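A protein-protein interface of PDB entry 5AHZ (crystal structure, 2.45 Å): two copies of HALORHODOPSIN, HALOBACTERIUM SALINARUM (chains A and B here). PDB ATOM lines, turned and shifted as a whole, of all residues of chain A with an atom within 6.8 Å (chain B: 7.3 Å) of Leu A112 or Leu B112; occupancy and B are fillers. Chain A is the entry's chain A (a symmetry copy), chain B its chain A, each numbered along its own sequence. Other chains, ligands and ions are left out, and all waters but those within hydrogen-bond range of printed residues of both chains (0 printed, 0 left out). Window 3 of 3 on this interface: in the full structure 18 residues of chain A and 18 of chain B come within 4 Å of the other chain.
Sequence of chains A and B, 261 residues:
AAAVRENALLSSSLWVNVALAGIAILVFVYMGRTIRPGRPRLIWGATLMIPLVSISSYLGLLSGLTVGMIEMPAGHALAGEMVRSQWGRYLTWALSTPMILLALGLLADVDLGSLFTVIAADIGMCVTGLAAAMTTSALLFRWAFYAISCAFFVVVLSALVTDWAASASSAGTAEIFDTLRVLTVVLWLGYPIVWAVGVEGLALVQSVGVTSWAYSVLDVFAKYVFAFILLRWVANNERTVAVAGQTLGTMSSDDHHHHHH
CD1 of Leu B42 touches CB of Asp A111, 3.9 Å away. Leu A112 touches Leu B112 (CD1 to CD1, 3.6 Å). Gly A113 touches Leu B42. Ser A114 touches Leu B42. Phe A116 touches Leu B115 (CE2 to CD2, 3.8 Å). Phe B116 touches Phe A116 (CE1 to CZ, 3.5 Å). Thr A117 touches Leu B102 (OG1 to CD2, 3.6 Å).
Hydrophobic or aromatic side chains of chain B within 4 Å of the printed part of chain A: Leu B42, Leu B102, Leu B112, Leu B115 and Phe B116. Hydrophobic or aromatic side chains of chain A that line the printed part of chain B: Leu A112 and Phe A116. Among the printed residues, 7 pairs touch across the chains.
Of chain B, only Leu B112 comes within 4 Å of Leu A112. Leu B112 touches just one residue of chain A: Leu A112. Of the printed residues of chain A, Leu B102 touches Thr A117 (3.6 Å). Of the printed residues of chain B, Thr A117 touches Leu B102.
Leu B112 touches its own counterpart, Leu A112. Phe A116 touches Leu B115, but with the chains exchanged Leu A115 does not touch Phe B116 (7.8 Å). Phe B116 touches its own counterpart, Phe A116. Of the 7 pairs that touch across the chains among the printed residues, 2 have their exchanged pair printed and touching as well.
O of Gly A113 sits at hydrogen-bond distance from OG1 of Thr A117 (3.1 Å).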
ATOM      1  N   VAL A 110       0.138  10.569  22.532  1.00  0.00           N
ATOM      2  CA  VAL A 110       0.534  10.117  23.858  1.00  0.00           C
ATOM      3  C   VAL A 110       1.891   9.412  23.864  1.00  0.00           C
ATOM      4  O   VAL A 110       2.435   9.071  22.818  1.00  0.00           O
ATOM      5  CB  VAL A 110      -0.521   9.157  24.449  1.00  0.00           C
ATOM      6  CG1 VAL A 110      -1.877   9.848  24.551  1.00  0.00           C
ATOM      7  CG2 VAL A 110      -0.611   7.884  23.607  1.00  0.00           C
ATOM      8  N   ASP A 111       2.433   9.203  25.058  1.00  0.00           N
ATOM      9  CA  ASP A 111       3.647   8.411  25.227  1.00  0.00           C
ATOM     10  C   ASP A 111       3.349   6.945  24.999  1.00  0.00           C
ATOM     11  O   ASP A 111       2.462   6.390  25.647  1.00  0.00           O
ATOM     12  CB  ASP A 111       4.225   8.588  26.629  1.00  0.00           C
ATOM     13  CG  ASP A 111       4.214  10.029  27.084  1.00  0.00           C
ATOM     14  OD1 ASP A 111       4.639  10.902  26.293  1.00  0.00           O
ATOM     15  OD2 ASP A 111       3.768  10.290  28.225  1.00  0.00           O
ATOM     16  N   LEU A 112       4.110   6.322  24.105  1.00  0.00           N
ATOM     17  CA  LEU A 112       3.938   4.914  23.763  1.00  0.00           C
ATOM     18  C   LEU A 112       3.844   4.002  24.982  1.00  0.00           C
ATOM     19  O   LEU A 112       3.252   2.927  24.920  1.00  0.00           O
ATOM     20  CB  LEU A 112       5.088   4.460  22.882  1.00  0.00           C
ATOM     21  CG  LEU A 112       5.265   5.341  21.653  1.00  0.00           C
ATOM     22  CD1 LEU A 112       6.682   5.205  21.132  1.00  0.00           C
ATOM     23  CD2 LEU A 112       4.241   4.991  20.568  1.00  0.00           C
ATOM     24  N   GLY A 113       4.436   4.430  26.087  1.00  0.00           N
ATOM     25  CA  GLY A 113       4.438   3.630  27.285  1.00  0.00           C
ATOM     26  C   GLY A 113       3.047   3.664  27.859  1.00  0.00           C
ATOM     27  O   GLY A 113       2.489   2.619  28.195  1.00  0.00           O
ATOM     28  N   SER A 114       2.489   4.868  27.973  1.00  0.00           N
ATOM     29  CA  SER A 114       1.106   5.019  28.380  1.00  0.00           C
ATOM     30  C   SER A 114       0.183   4.253  27.434  1.00  0.00           C
ATOM     31  O   SER A 114      -0.741   3.575  27.881  1.00  0.00           O
ATOM     32  CB  SER A 114       0.700   6.489  28.424  1.00  0.00           C
ATOM     33  OG  SER A 114      -0.692   6.610  28.693  1.00  0.00           O
ATOM     34  N   LEU A 115       0.446   4.358  26.136  1.00  0.00           N
ATOM     35  CA  LEU A 115      -0.325   3.628  25.146  1.00  0.00           C
ATOM     36  C   LEU A 115      -0.320   2.121  25.400  1.00  0.00           C
ATOM     37  O   LEU A 115      -1.371   1.476  25.395  1.00  0.00           O
ATOM     38  CB  LEU A 115       0.208   3.900  23.740  1.00  0.00           C
ATOM     39  CG  LEU A 115      -0.570   3.111  22.681  1.00  0.00           C
ATOM     40  CD1 LEU A 115      -1.973   3.711  22.485  1.00  0.00           C
ATOM     41  CD2 LEU A 115       0.193   2.990  21.360  1.00  0.00           C
ATOM     42  N   PHE A 116       0.861   1.570  25.632  1.00  0.00           N
ATOM     43  CA  PHE A 116       1.019   0.129  25.774  1.00  0.00           C
ATOM     44  C   PHE A 116       0.313  -0.379  27.020  1.00  0.00           C
ATOM     45  O   PHE A 116      -0.319  -1.445  27.000  1.00  0.00           O
ATOM     46  CB  PHE A 116       2.501  -0.252  25.820  1.00  0.00           C
ATOM     47  CG  PHE A 116       3.259   0.049  24.548  1.00  0.00           C
ATOM     48  CD1 PHE A 116       2.589   0.278  23.357  1.00  0.00           C
ATOM     49  CD2 PHE A 116       4.650   0.103  24.552  1.00  0.00           C
ATOM     50  CE1 PHE A 116       3.293   0.560  22.187  1.00  0.00           C
ATOM     51  CE2 PHE A 116       5.361   0.380  23.390  1.00  0.00           C
ATOM     52  CZ  PHE A 116       4.682   0.611  22.207  1.00  0.00           C
ATOM     53  N   THR A 117       0.418   0.388  28.100  1.00  0.00           N
ATOM     54  CA  THR A 117      -0.203   0.025  29.375  1.00  0.00           C
ATOM     55  C   THR A 117      -1.733   0.137  29.353  1.00  0.00           C
ATOM     56  O   THR A 117      -2.447  -0.698  29.931  1.00  0.00           O
ATOM     57  CB  THR A 117       0.341   0.905  30.525  1.00  0.00           C
ATOM     58  OG1 THR A 117       1.768   0.775  30.593  1.00  0.00           O
ATOM     59  CG2 THR A 117      -0.258   0.491  31.851  1.00  0.00           C
ATOM     60  N   LEU B  42       4.581   6.125  34.438  1.00  0.00           N
ATOM     61  CA  LEU B  42       4.442   5.104  33.404  1.00  0.00           C
ATOM     62  C   LEU B  42       4.924   3.749  33.929  1.00  0.00           C
ATOM     63  O   LEU B  42       4.302   2.718  33.669  1.00  0.00           O
ATOM     64  CB  LEU B  42       5.214   5.490  32.137  1.00  0.00           C
ATOM     65  CG  LEU B  42       4.717   6.661  31.263  1.00  0.00           C
ATOM     66  CD1 LEU B  42       5.159   6.473  29.824  1.00  0.00           C
ATOM     67  CD2 LEU B  42       3.205   6.880  31.326  1.00  0.00           C
ATOM     68  N   LEU B 102       7.661  -5.022  30.176  1.00  0.00           N
ATOM     69  CA  LEU B 102       7.375  -3.624  29.901  1.00  0.00           C
ATOM     70  C   LEU B 102       7.934  -2.720  31.009  1.00  0.00           C
ATOM     71  O   LEU B 102       8.583  -1.706  30.727  1.00  0.00           O
ATOM     72  CB  LEU B 102       5.874  -3.403  29.733  1.00  0.00           C
ATOM     73  CG  LEU B 102       5.482  -1.946  29.472  1.00  0.00           C
ATOM     74  CD1 LEU B 102       6.266  -1.342  28.284  1.00  0.00           C
ATOM     75  CD2 LEU B 102       3.969  -1.817  29.294  1.00  0.00           C
ATOM     76  N   LEU B 106      10.828  -0.056  30.367  1.00  0.00           N
ATOM     77  CA  LEU B 106      10.604   1.351  30.609  1.00  0.00           C
ATOM     78  C   LEU B 106      11.689   1.818  31.553  1.00  0.00           C
ATOM     79  O   LEU B 106      12.230   2.906  31.397  1.00  0.00           O
ATOM     80  CB  LEU B 106       9.211   1.603  31.193  1.00  0.00           C
ATOM     81  CG  LEU B 106       8.033   1.487  30.223  1.00  0.00           C
ATOM     82  CD1 LEU B 106       6.681   1.488  30.952  1.00  0.00           C
ATOM     83  CD2 LEU B 106       8.100   2.600  29.174  1.00  0.00           C
ATOM     84  N   ASP B 109      14.907   1.954  29.612  1.00  0.00           N
ATOM     85  CA  ASP B 109      14.772   2.824  28.440  1.00  0.00           C
ATOM     86  C   ASP B 109      15.302   2.174  27.151  1.00  0.00           C
ATOM     87  O   ASP B 109      16.230   2.683  26.525  1.00  0.00           O
ATOM     88  CB  ASP B 109      15.487   4.155  28.694  1.00  0.00           C
ATOM     89  CG  ASP B 109      15.197   5.187  27.619  1.00  0.00           C
ATOM     90  OD1 ASP B 109      14.058   5.192  27.092  1.00  0.00           O
ATOM     91  OD2 ASP B 109      16.111   5.981  27.296  1.00  0.00           O
ATOM     92  N   VAL B 110      14.697   1.058  26.757  1.00  0.00           N
ATOM     93  CA  VAL B 110      15.175   0.270  25.630  1.00  0.00           C
ATOM     94  C   VAL B 110      14.601   0.738  24.292  1.00  0.00           C
ATOM     95  O   VAL B 110      13.663   1.527  24.245  1.00  0.00           O
ATOM     96  CB  VAL B 110      14.830  -1.223  25.819  1.00  0.00           C
ATOM     97  CG1 VAL B 110      15.462  -1.762  27.097  1.00  0.00           C
ATOM     98  CG2 VAL B 110      13.314  -1.420  25.826  1.00  0.00           C
ATOM     99  N   ASP B 111      15.180   0.243  23.205  1.00  0.00           N
ATOM    100  CA  ASP B 111      14.644   0.480  21.870  1.00  0.00           C
ATOM    101  C   ASP B 111      13.371  -0.313  21.670  1.00  0.00           C
ATOM    102  O   ASP B 111      13.371  -1.531  21.848  1.00  0.00           O
ATOM    103  CB  ASP B 111      15.653   0.078  20.796  1.00  0.00           C
ATOM    104  CG  ASP B 111      17.057   0.533  21.120  1.00  0.00           C
ATOM    105  OD1 ASP B 111      17.223   1.717  21.494  1.00  0.00           O
ATOM    106  OD2 ASP B 111      17.991  -0.296  21.014  1.00  0.00           O
ATOM    107  N   LEU B 112      12.306   0.374  21.272  1.00  0.00           N
ATOM    108  CA  LEU B 112      11.003  -0.245  21.050  1.00  0.00           C
ATOM    109  C   LEU B 112      11.068  -1.503  20.190  1.00  0.00           C
ATOM    110  O   LEU B 112      10.210  -2.377  20.287  1.00  0.00           O
ATOM    111  CB  LEU B 112      10.067   0.759  20.400  1.00  0.00           C
ATOM    112  CG  LEU B 112       9.969   2.059  21.187  1.00  0.00           C
ATOM    113  CD1 LEU B 112       9.500   3.172  20.271  1.00  0.00           C
ATOM    114  CD2 LEU B 112       9.036   1.908  22.394  1.00  0.00           C
ATOM    115  N   GLY B 113      12.084  -1.588  19.344  1.00  0.00           N
ATOM    116  CA  GLY B 113      12.221  -2.719  18.461  1.00  0.00           C
ATOM    117  C   GLY B 113      12.642  -3.900  19.293  1.00  0.00           C
ATOM    118  O   GLY B 113      12.058  -4.978  19.182  1.00  0.00           O
ATOM    119  N   SER B 114      13.660  -3.696  20.127  1.00  0.00           N
ATOM    120  CA  SER B 114      14.069  -4.712  21.078  1.00  0.00           C
ATOM    121  C   SER B 114      12.899  -5.097  21.982  1.00  0.00           C
ATOM    122  O   SER B 114      12.678  -6.279  22.243  1.00  0.00           O
ATOM    123  CB  SER B 114      15.245  -4.236  21.924  1.00  0.00           C
ATOM    124  OG  SER B 114      15.541  -5.188  22.939  1.00  0.00           O
ATOM    125  N   LEU B 115      12.154  -4.099  22.446  1.00  0.00           N
ATOM    126  CA  LEU B 115      10.981  -4.347  23.265  1.00  0.00           C
ATOM    127  C   LEU B 115       9.974  -5.267  22.576  1.00  0.00           C
ATOM    128  O   LEU B 115       9.496  -6.237  23.167  1.00  0.00           O
ATOM    129  CB  LEU B 115      10.291  -3.034  23.629  1.00  0.00           C
ATOM    130  CG  LEU B 115       9.030  -3.274  24.466  1.00  0.00           C
ATOM    131  CD1 LEU B 115       9.404  -3.709  25.893  1.00  0.00           C
ATOM    132  CD2 LEU B 115       8.083  -2.071  24.461  1.00  0.00           C
ATOM    133  N   PHE B 116       9.665  -4.965  21.324  1.00  0.00           N
ATOM    134  CA  PHE B 116       8.635  -5.690  20.594  1.00  0.00           C
ATOM    135  C   PHE B 116       9.045  -7.133  20.355  1.00  0.00           C
ATOM    136  O   PHE B 116       8.221  -8.053  20.468  1.00  0.00           O
ATOM    137  CB  PHE B 116       8.333  -5.004  19.258  1.00  0.00           C
ATOM    138  CG  PHE B 116       7.745  -3.619  19.391  1.00  0.00           C
ATOM    139  CD1 PHE B 116       7.186  -3.193  20.586  1.00  0.00           C
ATOM    140  CD2 PHE B 116       7.756  -2.741  18.311  1.00  0.00           C
ATOM    141  CE1 PHE B 116       6.649  -1.913  20.704  1.00  0.00           C
ATOM    142  CE2 PHE B 116       7.219  -1.463  18.417  1.00  0.00           C
ATOM    143  CZ  PHE B 116       6.668  -1.048  19.616  1.00  0.00           C
ATOM    144  N   THR B 117      10.318  -7.328  20.033  1.00  0.00           N
ATOM    145  CA  THR B 117      10.859  -8.664  19.768  1.00  0.00           C
ATOM    146  C   THR B 117      10.967  -9.530  21.029  1.00  0.00           C
ATOM    147  O   THR B 117      10.702 -10.743  21.000  1.00  0.00           O
ATOM    148  CB  THR B 117      12.253  -8.574  19.105  1.00  0.00           C
ATOM    149  OG1 THR B 117      12.162  -7.808  17.897  1.00  0.00           O
ATOM    150  CG2 THR B 117      12.785  -9.953  18.779  1.00  0.00           C
ATOM    151  N   VAL B 118      11.364  -8.917  22.136  1.00  0.00           N
ATOM    152  CA  VAL B 118      11.451  -9.638  23.399  1.00  0.00           C
ATOM    153  C   VAL B 118      10.074 -10.127  23.788  1.00  0.00           C
ATOM    154  O   VAL B 118       9.862 -11.317  24.024  1.00  0.00           O
ATOM    155  CB  VAL B 118      12.021  -8.759  24.516  1.00  0.00           C
ATOM    156  CG1 VAL B 118      11.789  -9.398  25.873  1.00  0.00           C
ATOM    157  CG2 VAL B 118      13.494  -8.501  24.264  1.00  0.00           C
